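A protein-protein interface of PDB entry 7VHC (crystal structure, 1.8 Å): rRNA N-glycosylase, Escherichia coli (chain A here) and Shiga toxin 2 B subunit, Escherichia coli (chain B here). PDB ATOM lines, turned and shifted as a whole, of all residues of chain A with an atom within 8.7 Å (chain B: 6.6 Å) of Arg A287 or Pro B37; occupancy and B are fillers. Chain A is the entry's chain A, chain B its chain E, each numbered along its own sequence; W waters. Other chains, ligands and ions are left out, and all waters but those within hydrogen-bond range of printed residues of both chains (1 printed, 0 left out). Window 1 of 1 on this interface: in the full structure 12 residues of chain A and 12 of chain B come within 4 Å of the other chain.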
ATOM      1  N   THR A 280     -21.235  21.552  36.460  1.00  0.00           N
ATOM      2  CA  THR A 280     -20.437  20.896  35.420  1.00  0.00           C
ATOM      3  C   THR A 280     -21.337  20.190  34.405  1.00  0.00           C
ATOM      4  O   THR A 280     -21.174  20.335  33.175  1.00  0.00           O
ATOM      5  CB  THR A 280     -19.463  19.903  36.075  1.00  0.00           C
ATOM      6  OG1 THR A 280     -18.533  20.623  36.898  1.00  0.00           O
ATOM      7  CG2 THR A 280     -18.712  19.086  35.049  1.00  0.00           C
ATOM      8  N   ALA A 281     -22.300  19.416  34.908  1.00  0.00           N
ATOM      9  CA  ALA A 281     -23.230  18.742  34.010  1.00  0.00           C
ATOM     10  C   ALA A 281     -24.003  19.761  33.191  1.00  0.00           C
ATOM     11  O   ALA A 281     -24.131  19.621  31.968  1.00  0.00           O
ATOM     12  CB  ALA A 281     -24.184  17.853  34.805  1.00  0.00           C
ATOM     13  N   ALA A 282     -24.492  20.818  33.849  1.00  0.00           N
ATOM     14  CA  ALA A 282     -25.220  21.870  33.142  1.00  0.00           C
ATOM     15  C   ALA A 282     -24.383  22.451  32.018  1.00  0.00           C
ATOM     16  O   ALA A 282     -24.908  22.791  30.949  1.00  0.00           O
ATOM     17  CB  ALA A 282     -25.624  22.981  34.121  1.00  0.00           C
ATOM     18  N   ALA A 283     -23.070  22.552  32.236  1.00  0.00           N
ATOM     19  CA  ALA A 283     -22.205  23.193  31.261  1.00  0.00           C
ATOM     20  C   ALA A 283     -21.891  22.318  30.060  1.00  0.00           C
ATOM     21  O   ALA A 283     -21.389  22.850  29.059  1.00  0.00           O
ATOM     22  CB  ALA A 283     -20.897  23.641  31.916  1.00  0.00           C
ATOM     23  N   PHE A 284     -22.135  21.003  30.116  1.00  0.00           N
ATOM     24  CA  PHE A 284     -22.114  20.271  28.850  1.00  0.00           C
ATOM     25  C   PHE A 284     -23.484  19.773  28.384  1.00  0.00           C
ATOM     26  O   PHE A 284     -23.567  19.130  27.334  1.00  0.00           O
ATOM     27  CB  PHE A 284     -21.085  19.123  28.873  1.00  0.00           C
ATOM     28  CG  PHE A 284     -21.350  18.022  29.871  1.00  0.00           C
ATOM     29  CD1 PHE A 284     -22.187  16.958  29.553  1.00  0.00           C
ATOM     30  CD2 PHE A 284     -20.676  17.995  31.081  1.00  0.00           C
ATOM     31  CE1 PHE A 284     -22.390  15.902  30.448  1.00  0.00           C
ATOM     32  CE2 PHE A 284     -20.869  16.946  31.994  1.00  0.00           C
ATOM     33  CZ  PHE A 284     -21.729  15.898  31.683  1.00  0.00           C
ATOM     34  N   LEU A 285     -24.566  20.102  29.096  1.00  0.00           N
ATOM     35  CA  LEU A 285     -25.916  19.740  28.679  1.00  0.00           C
ATOM     36  C   LEU A 285     -26.697  20.952  28.191  1.00  0.00           C
ATOM     37  O   LEU A 285     -27.932  20.913  28.129  1.00  0.00           O
ATOM     38  CB  LEU A 285     -26.662  19.053  29.824  1.00  0.00           C
ATOM     39  CG  LEU A 285     -25.973  17.777  30.328  1.00  0.00           C
ATOM     40  CD1 LEU A 285     -26.666  17.229  31.567  1.00  0.00           C
ATOM     41  CD2 LEU A 285     -25.972  16.718  29.222  1.00  0.00           C
ATOM     42  N   ASN A 286     -25.999  22.038  27.869  1.00  0.00           N
ATOM     43  CA  ASN A 286     -26.638  23.260  27.404  1.00  0.00           C
ATOM     44  C   ASN A 286     -26.405  23.510  25.917  1.00  0.00           C
ATOM     45  O   ASN A 286     -26.542  24.650  25.468  1.00  0.00           O
ATOM     46  CB  ASN A 286     -26.141  24.453  28.219  1.00  0.00           C
ATOM     47  CG  ASN A 286     -24.694  24.763  27.957  1.00  0.00           C
ATOM     48  OD1 ASN A 286     -23.968  23.941  27.392  1.00  0.00           O
ATOM     49  ND2 ASN A 286     -24.256  25.960  28.357  1.00  0.00           N
ATOM     50  N   ARG A 287     -26.055  22.470  25.154  1.00  0.00           N
ATOM     51  CA  ARG A 287     -25.826  22.572  23.714  1.00  0.00           C
ATOM     52  C   ARG A 287     -27.112  22.261  22.955  1.00  0.00           C
ATOM     53  O   ARG A 287     -27.876  21.371  23.338  1.00  0.00           O
ATOM     54  CB  ARG A 287     -24.722  21.607  23.273  1.00  0.00           C
ATOM     55  CG  ARG A 287     -23.302  22.090  23.555  1.00  0.00           C
ATOM     56  CD  ARG A 287     -22.878  21.793  25.006  1.00  0.00           C
ATOM     57  NE  ARG A 287     -21.438  21.961  25.192  1.00  0.00           N
ATOM     58  CZ  ARG A 287     -20.855  23.064  25.650  1.00  0.00           C
ATOM     59  NH1 ARG A 287     -21.560  24.132  26.011  1.00  0.00           N
ATOM     60  NH2 ARG A 287     -19.525  23.112  25.720  1.00  0.00           N
ATOM     61  N   LYS A 288     -27.358  22.996  21.874  1.00  0.00           N
ATOM     62  CA  LYS A 288     -28.514  22.664  21.052  1.00  0.00           C
ATOM     63  C   LYS A 288     -28.105  21.611  20.022  1.00  0.00           C
ATOM     64  O   LYS A 288     -26.987  21.088  20.038  1.00  0.00           O
ATOM     65  CB  LYS A 288     -29.089  23.908  20.379  1.00  0.00           C
ATOM     66  CG  LYS A 288     -28.279  24.433  19.199  1.00  0.00           C
ATOM     67  CD  LYS A 288     -29.008  25.662  18.583  1.00  0.00           C
ATOM     68  CE  LYS A 288     -28.160  26.367  17.536  1.00  0.00           C
ATOM     69  NZ  LYS A 288     -28.905  27.465  16.845  1.00  0.00           N
ATOM     70  N   SER A 289     -29.019  21.285  19.117  1.00  0.00           N
ATOM     71  CA  SER A 289     -28.733  20.301  18.079  1.00  0.00           C
ATOM     72  C   SER A 289     -27.484  20.682  17.294  1.00  0.00           C
ATOM     73  O   SER A 289     -27.354  21.810  16.812  1.00  0.00           O
ATOM     74  CB  SER A 289     -29.936  20.186  17.148  1.00  0.00           C
ATOM     75  OG  SER A 289     -29.613  19.422  15.996  1.00  0.00           O
ATOM     76  N   GLN A 290     -26.566  19.729  17.170  1.00  0.00           N
ATOM     77  CA  GLN A 290     -25.246  20.025  16.624  1.00  0.00           C
ATOM     78  C   GLN A 290     -25.336  20.523  15.186  1.00  0.00           C
ATOM     79  O   GLN A 290     -24.644  21.475  14.808  1.00  0.00           O
ATOM     80  CB  GLN A 290     -24.370  18.775  16.706  1.00  0.00           C
ATOM     81  CG  GLN A 290     -22.942  18.956  16.205  1.00  0.00           C
ATOM     82  CD  GLN A 290     -22.024  19.501  17.282  1.00  0.00           C
ATOM     83  OE1 GLN A 290     -22.412  20.373  18.069  1.00  0.00           O
ATOM     84  NE2 GLN A 290     -20.792  19.004  17.314  1.00  0.00           N
ATOM     85  N   TYR A 293     -26.448  24.035  15.285  1.00  0.00           N
ATOM     86  CA  TYR A 293     -25.396  24.884  15.834  1.00  0.00           C
ATOM     87  C   TYR A 293     -24.363  25.230  14.774  1.00  0.00           C
ATOM     88  O   TYR A 293     -24.052  26.410  14.533  1.00  0.00           O
ATOM     89  CB  TYR A 293     -24.727  24.165  17.000  1.00  0.00           C
ATOM     90  CG  TYR A 293     -23.534  24.878  17.588  1.00  0.00           C
ATOM     91  CD1 TYR A 293     -23.705  25.952  18.451  1.00  0.00           C
ATOM     92  CD2 TYR A 293     -22.241  24.446  17.315  1.00  0.00           C
ATOM     93  CE1 TYR A 293     -22.607  26.599  19.019  1.00  0.00           C
ATOM     94  CE2 TYR A 293     -21.136  25.079  17.880  1.00  0.00           C
ATOM     95  CZ  TYR A 293     -21.328  26.148  18.734  1.00  0.00           C
ATOM     96  OH  TYR A 293     -20.242  26.779  19.319  1.00  0.00           O
ATOM     97  N   THR A 294     -23.827  24.206  14.121  1.00  0.00           N
ATOM     98  CA  THR A 294     -22.719  24.414  13.205  1.00  0.00           C
ATOM     99  C   THR A 294     -23.149  25.109  11.926  1.00  0.00           C
ATOM    100  O   THR A 294     -22.377  25.906  11.377  1.00  0.00           O
ATOM    101  CB  THR A 294     -22.046  23.071  12.933  1.00  0.00           C
ATOM    102  OG1 THR A 294     -21.497  22.604  14.162  1.00  0.00           O
ATOM    103  CG2 THR A 294     -20.962  23.174  11.851  1.00  0.00           C
ATOM    104  N   PHE B  19     -10.736  28.606  16.351  1.00  0.00           N
ATOM    105  CA  PHE B  19     -10.892  28.214  17.750  1.00  0.00           C
ATOM    106  C   PHE B  19      -9.597  27.524  18.161  1.00  0.00           C
ATOM    107  O   PHE B  19      -9.276  26.446  17.658  1.00  0.00           O
ATOM    108  CB  PHE B  19     -12.108  27.302  17.923  1.00  0.00           C
ATOM    109  CG  PHE B  19     -12.510  27.049  19.351  1.00  0.00           C
ATOM    110  CD1 PHE B  19     -13.275  27.983  20.047  1.00  0.00           C
ATOM    111  CD2 PHE B  19     -12.171  25.856  19.985  1.00  0.00           C
ATOM    112  CE1 PHE B  19     -13.676  27.736  21.352  1.00  0.00           C
ATOM    113  CE2 PHE B  19     -12.570  25.604  21.299  1.00  0.00           C
ATOM    114  CZ  PHE B  19     -13.319  26.547  21.980  1.00  0.00           C
ATOM    115  N   ARG B  32     -13.670  24.133  12.592  1.00  0.00           N
ATOM    116  CA  ARG B  32     -14.878  23.316  12.649  1.00  0.00           C
ATOM    117  C   ARG B  32     -15.708  23.734  13.859  1.00  0.00           C
ATOM    118  O   ARG B  32     -15.293  23.527  15.004  1.00  0.00           O
ATOM    119  CB  ARG B  32     -14.513  21.837  12.722  1.00  0.00           C
ATOM    120  CG  ARG B  32     -13.453  21.395  11.708  1.00  0.00           C
ATOM    121  CD  ARG B  32     -14.026  21.223  10.305  1.00  0.00           C
ATOM    122  NE  ARG B  32     -12.961  21.045   9.323  1.00  0.00           N
ATOM    123  CZ  ARG B  32     -12.672  19.889   8.744  1.00  0.00           C
ATOM    124  NH1 ARG B  32     -13.377  18.800   8.992  1.00  0.00           N
ATOM    125  NH2 ARG B  32     -11.638  19.820   7.910  1.00  0.00           N
ATOM    126  N   TRP B  33     -16.877  24.333  13.618  1.00  0.00           N
ATOM    127  CA  TRP B  33     -17.727  24.698  14.740  1.00  0.00           C
ATOM    128  C   TRP B  33     -18.188  23.470  15.503  1.00  0.00           C
ATOM    129  O   TRP B  33     -18.430  23.559  16.709  1.00  0.00           O
ATOM    130  CB  TRP B  33     -18.936  25.513  14.269  1.00  0.00           C
ATOM    131  CG  TRP B  33     -18.637  26.986  14.108  1.00  0.00           C
ATOM    132  CD1 TRP B  33     -17.426  27.561  13.817  1.00  0.00           C
ATOM    133  CD2 TRP B  33     -19.579  28.062  14.211  1.00  0.00           C
ATOM    134  NE1 TRP B  33     -17.558  28.939  13.739  1.00  0.00           N
ATOM    135  CE2 TRP B  33     -18.869  29.270  13.982  1.00  0.00           C
ATOM    136  CE3 TRP B  33     -20.944  28.124  14.492  1.00  0.00           C
ATOM    137  CZ2 TRP B  33     -19.494  30.526  14.010  1.00  0.00           C
ATOM    138  CZ3 TRP B  33     -21.565  29.382  14.520  1.00  0.00           C
ATOM    139  CH2 TRP B  33     -20.836  30.559  14.281  1.00  0.00           C
ATOM    140  N   ASN B  34     -18.333  22.323  14.822  1.00  0.00           N
ATOM    141  CA  ASN B  34     -18.652  21.084  15.534  1.00  0.00           C
ATOM    142  C   ASN B  34     -17.724  20.882  16.722  1.00  0.00           C
ATOM    143  O   ASN B  34     -18.143  20.391  17.768  1.00  0.00           O
ATOM    144  CB  ASN B  34     -18.522  19.868  14.608  1.00  0.00           C
ATOM    145  CG  ASN B  34     -19.751  19.625  13.758  1.00  0.00           C
ATOM    146  OD1 ASN B  34     -20.838  20.124  14.050  1.00  0.00           O
ATOM    147  ND2 ASN B  34     -19.570  18.874  12.669  1.00  0.00           N
ATOM    148  N   LEU B  35     -16.447  21.229  16.566  1.00  0.00           N
ATOM    149  CA  LEU B  35     -15.480  20.956  17.620  1.00  0.00           C
ATOM    150  C   LEU B  35     -15.529  21.951  18.776  1.00  0.00           C
ATOM    151  O   LEU B  35     -14.981  21.658  19.852  1.00  0.00           O
ATOM    152  CB  LEU B  35     -14.075  20.921  17.019  1.00  0.00           C
ATOM    153  CG  LEU B  35     -13.773  19.550  16.412  1.00  0.00           C
ATOM    154  CD1 LEU B  35     -12.473  19.612  15.620  1.00  0.00           C
ATOM    155  CD2 LEU B  35     -13.699  18.500  17.512  1.00  0.00           C
ATOM    156  N   GLN B  36     -16.180  23.105  18.615  1.00  0.00           N
ATOM    157  CA  GLN B  36     -16.160  24.070  19.715  1.00  0.00           C
ATOM    158  C   GLN B  36     -16.847  23.540  20.970  1.00  0.00           C
ATOM    159  O   GLN B  36     -16.201  23.528  22.032  1.00  0.00           O
ATOM    160  CB  GLN B  36     -16.742  25.408  19.250  1.00  0.00           C
ATOM    161  CG  GLN B  36     -15.848  26.079  18.200  1.00  0.00           C
ATOM    162  CD  GLN B  36     -16.222  27.519  17.931  1.00  0.00           C
ATOM    163  OE1 GLN B  36     -16.862  28.177  18.756  1.00  0.00           O
ATOM    164  NE2 GLN B  36     -15.782  28.036  16.775  1.00  0.00           N
ATOM    165  N   PRO B  37     -18.104  23.083  20.939  1.00  0.00           N
ATOM    166  CA  PRO B  37     -18.692  22.552  22.183  1.00  0.00           C
ATOM    167  C   PRO B  37     -17.995  21.296  22.652  1.00  0.00           C
ATOM    168  O   PRO B  37     -17.856  21.085  23.857  1.00  0.00           O
ATOM    169  CB  PRO B  37     -20.152  22.276  21.796  1.00  0.00           C
ATOM    170  CG  PRO B  37     -20.131  22.148  20.314  1.00  0.00           C
ATOM    171  CD  PRO B  37     -19.079  23.083  19.834  1.00  0.00           C
ATOM    172  N   LEU B  38     -17.549  20.454  21.723  1.00  0.00           N
ATOM    173  CA  LEU B  38     -16.863  19.224  22.111  1.00  0.00           C
ATOM    174  C   LEU B  38     -15.570  19.543  22.842  1.00  0.00           C
ATOM    175  O   LEU B  38     -15.293  18.999  23.919  1.00  0.00           O
ATOM    176  CB  LEU B  38     -16.590  18.369  20.874  1.00  0.00           C
ATOM    177  CG  LEU B  38     -17.819  17.948  20.078  1.00  0.00           C
ATOM    178  CD1 LEU B  38     -17.374  17.179  18.835  1.00  0.00           C
ATOM    179  CD2 LEU B  38     -18.745  17.098  20.929  1.00  0.00           C
ATOM    180  N   LEU B  39     -14.784  20.466  22.287  1.00  0.00           N
ATOM    181  CA  LEU B  39     -13.529  20.836  22.929  1.00  0.00           C
ATOM    182  C   LEU B  39     -13.774  21.581  24.233  1.00  0.00           C
ATOM    183  O   LEU B  39     -13.064  21.358  25.213  1.00  0.00           O
ATOM    184  CB  LEU B  39     -12.679  21.673  21.974  1.00  0.00           C
ATOM    185  CG  LEU B  39     -12.047  20.932  20.790  1.00  0.00           C
ATOM    186  CD1 LEU B  39     -11.503  21.938  19.783  1.00  0.00           C
ATOM    187  CD2 LEU B  39     -10.925  19.990  21.261  1.00  0.00           C
ATOM    188  N   GLN B  40     -14.765  22.479  24.279  1.00  0.00           N
ATOM    189  CA  GLN B  40     -14.977  23.199  25.530  1.00  0.00           C
ATOM    190  C   GLN B  40     -15.491  22.271  26.626  1.00  0.00           C
ATOM    191  O   GLN B  40     -15.089  22.394  27.788  1.00  0.00           O
ATOM    192  CB  GLN B  40     -15.927  24.378  25.340  1.00  0.00           C
ATOM    193  CG  GLN B  40     -15.911  25.236  26.622  1.00  0.00           C
ATOM    194  CD  GLN B  40     -17.133  26.081  26.788  1.00  0.00           C
ATOM    195  OE1 GLN B  40     -18.257  25.601  26.652  1.00  0.00           O
ATOM    196  NE2 GLN B  40     -16.925  27.360  27.113  1.00  0.00           N
ATOM    197  N   SER B  41     -16.385  21.342  26.287  1.00  0.00           N
ATOM    198  CA  SER B  41     -16.818  20.361  27.274  1.00  0.00           C
ATOM    199  C   SER B  41     -15.641  19.522  27.751  1.00  0.00           C
ATOM    200  O   SER B  41     -15.513  19.247  28.952  1.00  0.00           O
ATOM    201  CB  SER B  41     -17.914  19.478  26.683  1.00  0.00           C
ATOM    202  OG  SER B  41     -19.094  20.227  26.460  1.00  0.00           O
ATOM    203  N   ALA B  42     -14.766  19.114  26.823  1.00  0.00           N
ATOM    204  CA  ALA B  42     -13.545  18.414  27.218  1.00  0.00           C
ATOM    205  C   ALA B  42     -12.721  19.259  28.179  1.00  0.00           C
ATOM    206  O   ALA B  42     -12.182  18.745  29.160  1.00  0.00           O
ATOM    207  CB  ALA B  42     -12.723  18.063  25.972  1.00  0.00           C
ATOM    208  N   LEU B  44     -13.744  21.723  30.268  1.00  0.00           N
ATOM    209  CA  LEU B  44     -14.339  21.964  31.570  1.00  0.00           C
ATOM    210  C   LEU B  44     -14.524  20.688  32.375  1.00  0.00           C
ATOM    211  O   LEU B  44     -14.694  20.772  33.594  1.00  0.00           O
ATOM    212  CB  LEU B  44     -15.674  22.690  31.423  1.00  0.00           C
ATOM    213  CG  LEU B  44     -16.872  22.019  30.758  1.00  0.00           C
ATOM    214  CD1 LEU B  44     -17.752  21.367  31.822  1.00  0.00           C
ATOM    215  CD2 LEU B  44     -17.667  23.104  30.028  1.00  0.00           C
HETATM  216  O   HOH W   1     -20.594  19.016  24.466  1.00  0.00           O
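NH2 of Arg A287 is in hydrogen-bond range of OG of Ser B41 (3.0 Å).
The guanidinium group of Arg A287 is in hydrogen-bond range of the side-chain amide oxygen of Gln B40 (2.9 Å).
O of Asn B34 is in hydrogen-bond range of NE2 of Gln A290 (3.0 Å).
The guanidinium group (NH2) of Arg A287 lies within hydrogen-bond range of the backbone carbonyl oxygen (O) of Pro B37 (3.2 Å).
OG1 of Thr A294 is in hydrogen-bond range of OD1 of Asn B34 (2.6 Å).
The guanidinium group of Arg A287 is in hydrogen-bond range of the backbone carbonyl oxygen of Ala A283 (3.3 Å).
O of Ala A283 sits close to OD1 of Asn A286 (3.3 Å).
O of Gln A290 lies within hydrogen-bond range of OG1 of Thr A294, 3.4 Å away.
OG of Ser B41 lies within hydrogen-bond range of O of Pro B37 (3.0 Å).
The guanidinium group (NH1) of Arg A287 sits at hydrogen-bond distance from the side-chain amide oxygen (OD1) of Asn A286 (2.8 Å).
Leu B44 touches Thr A280 (CD1 to O, 3.8 Å).
CB of Ala A283 touches CD2 of Leu B44 (3.8 Å).
Phe A284 touches Ser B41.
Gln A290 touches Pro B37.
Trp B33 touches Tyr A293.
Gln B36 touches Tyr A293.
CE2 of Tyr A293 touches CD of Pro B37, 3.5 Å away.
Trp B33 touches Thr A294 (C to OG1, 3.7 Å).
Of the printed residues of chain B, Thr A280 touches Leu B44 (3.8 Å).
Ala A282 touches none of the printed residues of chain B.
Arg A287 touches just these residues of chain B: Pro B37 (3.2 Å), Gln B40 (2.9 Å) and Ser B41 (3.0 Å).
Lys A288 touches none of the printed residues of chain B.
Printed residues of chain A within 4 Å of Gln B36: Tyr A293 (3.7 Å).
Of chain A, only Arg A287 (3.2 Å), Gln A290 (3.7 Å) and Tyr A293 (3.5 Å) come within 4 Å of Pro B37.
Of the printed residues of chain A, Gln B40 touches Arg A287 (2.9 Å).
Of the printed residues of chain A, Ser B41 touches Phe A284 (3.3 Å) and Arg A287 (3.0 Å).
The nearest printed residue of chain B that does not touch Thr A294 is Arg B32 (5.7 Å).
Along chain A the printed residues that touch a printed residue of chain B span positions 280 to 294.
Hydrophobic or aromatic side chains of chain B that line the printed part of chain A: Trp B33, Pro B37 and Leu B44.
Among the printed residues, 13 pairs touch across the chains.
Water W1 lies within hydrogen-bond range of the side-chain hydroxyl (OG) of Ser B41 (2.8 Å), the guanidinium group (NE) of Arg A287 (3.1 Å) and the backbone carbonyl oxygen (O) of Pro B37 (3.5 Å).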
